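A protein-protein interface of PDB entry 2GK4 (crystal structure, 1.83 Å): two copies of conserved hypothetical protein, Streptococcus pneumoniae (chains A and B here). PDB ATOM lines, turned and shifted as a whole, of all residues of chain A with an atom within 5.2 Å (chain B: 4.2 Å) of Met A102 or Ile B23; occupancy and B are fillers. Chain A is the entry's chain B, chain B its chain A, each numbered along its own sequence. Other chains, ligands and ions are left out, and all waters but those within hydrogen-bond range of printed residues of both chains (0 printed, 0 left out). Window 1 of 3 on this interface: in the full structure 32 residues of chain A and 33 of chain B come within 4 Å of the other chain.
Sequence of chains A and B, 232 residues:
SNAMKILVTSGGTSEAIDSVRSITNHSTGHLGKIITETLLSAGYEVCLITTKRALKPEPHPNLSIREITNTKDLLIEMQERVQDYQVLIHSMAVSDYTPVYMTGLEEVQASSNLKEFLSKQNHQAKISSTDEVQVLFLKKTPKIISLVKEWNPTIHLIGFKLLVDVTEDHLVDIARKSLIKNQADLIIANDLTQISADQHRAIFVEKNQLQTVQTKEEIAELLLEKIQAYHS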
ATOM      1  N   ILE A  17     -11.688 -22.210  14.741  1.00  0.00           N
ATOM      2  CA  ILE A  17     -10.492 -23.005  15.003  1.00  0.00           C
ATOM      3  C   ILE A  17     -10.898 -24.139  15.959  1.00  0.00           C
ATOM      4  O   ILE A  17     -10.516 -25.304  15.785  1.00  0.00           O
ATOM      5  CB  ILE A  17      -9.380 -22.144  15.648  1.00  0.00           C
ATOM      6  CG1 ILE A  17      -8.847 -21.102  14.653  1.00  0.00           C
ATOM      7  CG2 ILE A  17      -8.230 -23.030  16.210  1.00  0.00           C
ATOM      8  CD1 ILE A  17      -8.327 -19.849  15.378  1.00  0.00           C
ATOM      9  N   ARG A  21     -12.395 -20.428  19.806  1.00  0.00           N
ATOM     10  CA  ARG A  21     -11.700 -19.410  18.956  1.00  0.00           C
ATOM     11  C   ARG A  21     -12.082 -19.525  17.495  1.00  0.00           C
ATOM     12  O   ARG A  21     -12.357 -20.630  17.017  1.00  0.00           O
ATOM     13  CB  ARG A  21     -10.196 -19.670  18.991  1.00  0.00           C
ATOM     14  CG  ARG A  21      -9.474 -19.329  20.296  1.00  0.00           C
ATOM     15  CD  ARG A  21      -8.154 -20.109  20.345  1.00  0.00           C
ATOM     16  NE  ARG A  21      -8.430 -21.417  20.901  1.00  0.00           N
ATOM     17  CZ  ARG A  21      -8.423 -21.712  22.203  1.00  0.00           C
ATOM     18  NH1 ARG A  21      -8.081 -20.803  23.123  1.00  0.00           N
ATOM     19  NH2 ARG A  21      -8.750 -22.935  22.581  1.00  0.00           N
ATOM     20  N   SER A  22     -12.027 -18.396  16.779  1.00  0.00           N
ATOM     21  CA  SER A  22     -12.265 -18.379  15.339  1.00  0.00           C
ATOM     22  C   SER A  22     -11.283 -17.397  14.722  1.00  0.00           C
ATOM     23  O   SER A  22     -10.822 -16.484  15.405  1.00  0.00           O
ATOM     24  CB  SER A  22     -13.679 -17.867  15.039  1.00  0.00           C
ATOM     25  OG  SER A  22     -14.669 -18.807  15.378  1.00  0.00           O
ATOM     26  N   ILE A  23     -10.962 -17.576  13.442  1.00  0.00           N
ATOM     27  CA  ILE A  23     -10.343 -16.469  12.697  1.00  0.00           C
ATOM     28  C   ILE A  23     -11.488 -15.652  12.080  1.00  0.00           C
ATOM     29  O   ILE A  23     -12.319 -16.205  11.344  1.00  0.00           O
ATOM     30  CB  ILE A  23      -9.407 -16.981  11.581  1.00  0.00           C
ATOM     31  CG1 ILE A  23      -8.295 -17.844  12.171  1.00  0.00           C
ATOM     32  CG2 ILE A  23      -8.839 -15.738  10.806  1.00  0.00           C
ATOM     33  CD1 ILE A  23      -7.455 -17.073  13.248  1.00  0.00           C
ATOM     34  N   THR A  24     -11.554 -14.353  12.393  1.00  0.00           N
ATOM     35  CA  THR A  24     -12.645 -13.501  11.937  1.00  0.00           C
ATOM     36  C   THR A  24     -12.093 -12.430  10.991  1.00  0.00           C
ATOM     37  O   THR A  24     -10.959 -12.010  11.136  1.00  0.00           O
ATOM     38  CB  THR A  24     -13.377 -12.839  13.128  1.00  0.00           C
ATOM     39  OG1 THR A  24     -12.424 -12.092  13.911  1.00  0.00           O
ATOM     40  CG2 THR A  24     -14.009 -13.932  14.043  1.00  0.00           C
ATOM     41  N   VAL A 100      -5.813 -24.756  10.320  1.00  0.00           N
ATOM     42  CA  VAL A 100      -5.768 -26.216  10.237  1.00  0.00           C
ATOM     43  C   VAL A 100      -5.441 -26.873  11.589  1.00  0.00           C
ATOM     44  O   VAL A 100      -6.120 -27.826  12.012  1.00  0.00           O
ATOM     45  CB  VAL A 100      -4.774 -26.708   9.134  1.00  0.00           C
ATOM     46  CG1 VAL A 100      -4.652 -28.218   9.151  1.00  0.00           C
ATOM     47  CG2 VAL A 100      -5.251 -26.247   7.764  1.00  0.00           C
ATOM     48  N   TYR A 101      -4.427 -26.358  12.284  1.00  0.00           N
ATOM     49  CA  TYR A 101      -3.968 -26.993  13.516  1.00  0.00           C
ATOM     50  C   TYR A 101      -3.321 -25.963  14.427  1.00  0.00           C
ATOM     51  O   TYR A 101      -2.587 -25.106  13.945  1.00  0.00           O
ATOM     52  CB  TYR A 101      -2.968 -28.105  13.180  1.00  0.00           C
ATOM     53  CG  TYR A 101      -2.622 -29.014  14.339  1.00  0.00           C
ATOM     54  CD1 TYR A 101      -1.319 -29.095  14.821  1.00  0.00           C
ATOM     55  CD2 TYR A 101      -3.607 -29.792  14.954  1.00  0.00           C
ATOM     56  CE1 TYR A 101      -1.005 -29.938  15.891  1.00  0.00           C
ATOM     57  CE2 TYR A 101      -3.304 -30.617  16.018  1.00  0.00           C
ATOM     58  CZ  TYR A 101      -2.006 -30.679  16.486  1.00  0.00           C
ATOM     59  OH  TYR A 101      -1.704 -31.519  17.540  1.00  0.00           O
ATOM     60  N   MET A 102      -3.629 -26.016  15.723  1.00  0.00           N
ATOM     61  CA  MET A 102      -3.000 -25.119  16.691  1.00  0.00           C
ATOM     62  C   MET A 102      -2.360 -25.968  17.760  1.00  0.00           C
ATOM     63  O   MET A 102      -3.013 -26.834  18.322  1.00  0.00           O
ATOM     64  CB  MET A 102      -4.002 -24.124  17.328  1.00  0.00           C
ATOM     65  CG  MET A 102      -3.316 -22.853  17.957  1.00  0.00           C
ATOM     66  SD  MET A 102      -4.583 -21.378  18.338  1.00  0.00           S
ATOM     67  CE  MET A 102      -5.514 -21.304  16.783  1.00  0.00           C
ATOM     68  N   THR A 103      -1.081 -25.722  18.038  1.00  0.00           N
ATOM     69  CA  THR A 103      -0.375 -26.525  19.022  1.00  0.00           C
ATOM     70  C   THR A 103       0.748 -25.752  19.735  1.00  0.00           C
ATOM     71  O   THR A 103       1.076 -24.644  19.340  1.00  0.00           O
ATOM     72  CB  THR A 103       0.144 -27.829  18.378  1.00  0.00           C
ATOM     73  OG1 THR A 103       0.528 -28.747  19.410  1.00  0.00           O
ATOM     74  CG2 THR A 103       1.317 -27.547  17.402  1.00  0.00           C
ATOM     75  N   GLY A 104       1.304 -26.325  20.801  1.00  0.00           N
ATOM     76  CA  GLY A 104       2.412 -25.683  21.517  1.00  0.00           C
ATOM     77  C   GLY A 104       3.694 -25.667  20.688  1.00  0.00           C
ATOM     78  O   GLY A 104       3.920 -26.547  19.868  1.00  0.00           O
ATOM     79  N   GLN A 134       1.976 -20.648  21.479  1.00  0.00           N
ATOM     80  CA  GLN A 134       1.192 -21.466  20.566  1.00  0.00           C
ATOM     81  C   GLN A 134       1.550 -21.147  19.127  1.00  0.00           C
ATOM     82  O   GLN A 134       2.049 -20.053  18.826  1.00  0.00           O
ATOM     83  CB  GLN A 134      -0.302 -21.251  20.785  1.00  0.00           C
ATOM     84  CG  GLN A 134      -0.814 -21.748  22.112  1.00  0.00           C
ATOM     85  CD  GLN A 134      -0.873 -23.259  22.230  1.00  0.00           C
ATOM     86  OE1 GLN A 134      -0.318 -23.842  23.171  1.00  0.00           O
ATOM     87  NE2 GLN A 134      -1.573 -23.892  21.317  1.00  0.00           N
ATOM     88  N   VAL A 135       1.326 -22.124  18.255  1.00  0.00           N
ATOM     89  CA  VAL A 135       1.623 -22.002  16.833  1.00  0.00           C
ATOM     90  C   VAL A 135       0.379 -22.431  16.061  1.00  0.00           C
ATOM     91  O   VAL A 135      -0.142 -23.513  16.288  1.00  0.00           O
ATOM     92  CB  VAL A 135       2.826 -22.909  16.424  1.00  0.00           C
ATOM     93  CG1 VAL A 135       3.182 -22.716  14.968  1.00  0.00           C
ATOM     94  CG2 VAL A 135       4.036 -22.652  17.328  1.00  0.00           C
ATOM     95  N   LEU A 136      -0.095 -21.578  15.157  1.00  0.00           N
ATOM     96  CA  LEU A 136      -1.287 -21.875  14.377  1.00  0.00           C
ATOM     97  C   LEU A 136      -0.862 -22.062  12.929  1.00  0.00           C
ATOM     98  O   LEU A 136      -0.217 -21.187  12.361  1.00  0.00           O
ATOM     99  CB  LEU A 136      -2.258 -20.703  14.446  1.00  0.00           C
ATOM    100  CG  LEU A 136      -3.776 -20.860  14.210  1.00  0.00           C
ATOM    101  CD1 LEU A 136      -4.336 -19.642  13.483  1.00  0.00           C
ATOM    102  CD2 LEU A 136      -4.262 -22.156  13.594  1.00  0.00           C
ATOM    103  N   PHE A 137      -1.201 -23.210  12.365  1.00  0.00           N
ATOM    104  CA  PHE A 137      -0.950 -23.460  10.941  1.00  0.00           C
ATOM    105  C   PHE A 137      -2.214 -23.195  10.136  1.00  0.00           C
ATOM    106  O   PHE A 137      -3.284 -23.712  10.465  1.00  0.00           O
ATOM    107  CB  PHE A 137      -0.498 -24.909  10.719  1.00  0.00           C
ATOM    108  CG  PHE A 137       0.830 -25.234  11.341  1.00  0.00           C
ATOM    109  CD1 PHE A 137       0.916 -25.605  12.674  1.00  0.00           C
ATOM    110  CD2 PHE A 137       2.007 -25.188  10.576  1.00  0.00           C
ATOM    111  CE1 PHE A 137       2.173 -25.893  13.261  1.00  0.00           C
ATOM    112  CE2 PHE A 137       3.259 -25.491  11.155  1.00  0.00           C
ATOM    113  CZ  PHE A 137       3.333 -25.850  12.490  1.00  0.00           C
ATOM    114  N   SER B  14     -10.987 -10.149  20.925  1.00  0.00           N
ATOM    115  CA  SER B  14     -10.501 -10.351  19.565  1.00  0.00           C
ATOM    116  C   SER B  14      -9.085  -9.796  19.513  1.00  0.00           C
ATOM    117  O   SER B  14      -8.855  -8.654  19.908  1.00  0.00           O
ATOM    118  CB  SER B  14     -11.355  -9.581  18.549  1.00  0.00           C
ATOM    119  OG  SER B  14     -12.570 -10.257  18.244  1.00  0.00           O
ATOM    120  N   GLU B  15      -8.148 -10.596  19.026  1.00  0.00           N
ATOM    121  CA  GLU B  15      -6.748 -10.168  18.963  1.00  0.00           C
ATOM    122  C   GLU B  15      -6.354  -9.990  17.482  1.00  0.00           C
ATOM    123  O   GLU B  15      -6.370 -10.954  16.726  1.00  0.00           O
ATOM    124  CB  GLU B  15      -5.869 -11.226  19.645  1.00  0.00           C
ATOM    125  CG  GLU B  15      -6.271 -11.560  21.090  1.00  0.00           C
ATOM    126  CD  GLU B  15      -6.072 -10.407  22.056  1.00  0.00           C
ATOM    127  OE1 GLU B  15      -4.993  -9.742  22.000  1.00  0.00           O
ATOM    128  OE2 GLU B  15      -6.989 -10.188  22.885  1.00  0.00           O
ATOM    129  N   ILE B  17      -4.642  -9.829  13.967  1.00  0.00           N
ATOM    130  CA  ILE B  17      -3.521 -10.450  13.264  1.00  0.00           C
ATOM    131  C   ILE B  17      -2.944  -9.434  12.284  1.00  0.00           C
ATOM    132  O   ILE B  17      -1.723  -9.222  12.202  1.00  0.00           O
ATOM    133  CB  ILE B  17      -3.965 -11.721  12.507  1.00  0.00           C
ATOM    134  CG1 ILE B  17      -4.281 -12.837  13.509  1.00  0.00           C
ATOM    135  CG2 ILE B  17      -2.866 -12.199  11.562  1.00  0.00           C
ATOM    136  CD1 ILE B  17      -5.068 -14.010  12.904  1.00  0.00           C
ATOM    137  N   SER B  22      -8.554 -11.209  12.692  1.00  0.00           N
ATOM    138  CA  SER B  22      -8.275 -11.347  14.130  1.00  0.00           C
ATOM    139  C   SER B  22      -8.451 -12.781  14.538  1.00  0.00           C
ATOM    140  O   SER B  22      -9.131 -13.537  13.817  1.00  0.00           O
ATOM    141  CB  SER B  22      -9.296 -10.507  14.895  1.00  0.00           C
ATOM    142  OG  SER B  22      -9.019  -9.121  14.671  1.00  0.00           O
ATOM    143  N   ILE B  23      -7.833 -13.176  15.652  1.00  0.00           N
ATOM    144  CA  ILE B  23      -8.219 -14.446  16.265  1.00  0.00           C
ATOM    145  C   ILE B  23      -9.094 -14.062  17.447  1.00  0.00           C
ATOM    146  O   ILE B  23      -8.696 -13.275  18.331  1.00  0.00           O
ATOM    147  CB  ILE B  23      -7.011 -15.297  16.696  1.00  0.00           C
ATOM    148  CG1 ILE B  23      -7.483 -16.568  17.412  1.00  0.00           C
ATOM    149  CG2 ILE B  23      -5.987 -14.479  17.538  1.00  0.00           C
ATOM    150  CD1 ILE B  23      -6.346 -17.612  17.528  1.00  0.00           C
ATOM    151  N   THR B  24     -10.291 -14.626  17.457  1.00  0.00           N
ATOM    152  CA  THR B  24     -11.371 -14.069  18.280  1.00  0.00           C
ATOM    153  C   THR B  24     -11.943 -15.205  19.125  1.00  0.00           C
ATOM    154  O   THR B  24     -12.170 -16.314  18.596  1.00  0.00           O
ATOM    155  CB  THR B  24     -12.478 -13.521  17.358  1.00  0.00           C
ATOM    156  OG1 THR B  24     -11.979 -12.404  16.601  1.00  0.00           O
ATOM    157  CG2 THR B  24     -13.698 -13.083  18.157  1.00  0.00           C
ATOM    158  N   PRO B  99      -1.412 -12.795  18.984  1.00  0.00           N
ATOM    159  CA  PRO B  99      -0.470 -12.877  17.878  1.00  0.00           C
ATOM    160  C   PRO B  99       0.829 -12.124  18.140  1.00  0.00           C
ATOM    161  O   PRO B  99       0.816 -11.024  18.720  1.00  0.00           O
ATOM    162  CB  PRO B  99      -1.227 -12.189  16.730  1.00  0.00           C
ATOM    163  CG  PRO B  99      -2.644 -12.486  17.014  1.00  0.00           C
ATOM    164  CD  PRO B  99      -2.739 -12.317  18.520  1.00  0.00           C
ATOM    165  N   LEU B 138       1.982 -17.218  18.659  1.00  0.00           N
ATOM    166  CA  LEU B 138       1.207 -16.446  19.629  1.00  0.00           C
ATOM    167  C   LEU B 138       1.832 -16.636  20.995  1.00  0.00           C
ATOM    168  O   LEU B 138       2.322 -17.746  21.308  1.00  0.00           O
ATOM    169  CB  LEU B 138      -0.242 -16.917  19.659  1.00  0.00           C
ATOM    170  CG  LEU B 138      -1.042 -16.898  18.348  1.00  0.00           C
ATOM    171  CD1 LEU B 138      -0.894 -18.224  17.593  1.00  0.00           C
ATOM    172  CD2 LEU B 138      -2.492 -16.601  18.664  1.00  0.00           C
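O of Thr B24 lies within hydrogen-bond range of N of Ser A22 (2.8 Å). The backbone carbonyl oxygen (O) of Ser B22 is in hydrogen-bond range of the backbone NH (N) of Thr A24 (2.9 Å). OG1 of Thr B24 sits at hydrogen-bond distance from OG1 of Thr A24, at 2.7 Å. The backbone NH (N) of Leu B138 is in hydrogen-bond range of the backbone carbonyl oxygen (O) of Gln A134 (2.8 Å).
OG of Ser B14 lies within hydrogen-bond range of OG1 of Thr B24. The backbone carbonyl oxygen of Thr A103 sits close to the side-chain amide nitrogen of Gln A134, at 3.4 Å. The backbone NH of Glu B15 lies within hydrogen-bond range of the backbone carbonyl oxygen of Ile B23, at 2.8 Å.
Among the printed residues, merely in contact across the chains: Arg A21 with Thr B24 (3.2 Å), Ile A23 with Ser B22 (3.4 Å), Ser A22 with Ile B23 (3.4 Å), Ile A17 with Ile B23 (3.7 Å), Ser A22 with Ser B22 (3.8 Å), Met A102 with Ile B23 (3.9 Å), Ile A23 with Ile B17 (3.9 Å) and Ile A23 with Ile B23 (3.9 Å).
Printed residues of chain B within 4 Å of Ile A17: Ile B23 (3.7 Å). Of the printed residues of chain B, Thr A24 touches Ser B22 (2.9 Å) and Thr B24 (2.7 Å). Of chain B, only Ile B23 (3.9 Å) comes within 4 Å of Met A102. Printed residues of chain B within 4 Å of Gln A134: Leu B138 (2.8 Å). Phe A137 touches none of the printed residues of chain B. Of the printed residues of chain A, Ile B17 touches Ile A23 (3.9 Å). Printed residues of chain A within 4 Å of Ser B22: Ser A22 (3.8 Å), Ile A23 (3.4 Å) and Thr A24 (2.9 Å). The nearest residue of chain A that does not touch Ile B23 is Arg A21 (4.2 Å).
Of the 14 printed residues of chain A, 7 touch a printed residue of chain B. Hydrophobic or aromatic side chains of chain A that line the printed part of chain B: Ile A17, Ile A23 and Met A102. Hydrophobic or aromatic side chains of chain B within 4 Å of the printed part of chain A: Ile B17, Ile B23 and Leu B138. Among the printed residues, 12 pairs touch across the chains. Among the printed residues, no Asp or Glu carboxylate lies within 4 Å of a Lys or Arg side-chain nitrogen of the other chain.
Ile A17 touches Ile B23, and with the chains exchanged Ile A23 touches Ile B17. Ser B22 touches its own counterpart, Ser A22. Ser A22 touches Ile B23, and with the chains exchanged Ile A23 touches Ser B22. Ile A23 touches its own counterpart, Ile B23. Positions printed for both chains: 17, 22, 23 and 24. Of the 12 pairs that touch across the chains among the printed residues, 9 have their exchanged pair printed and touching as well.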
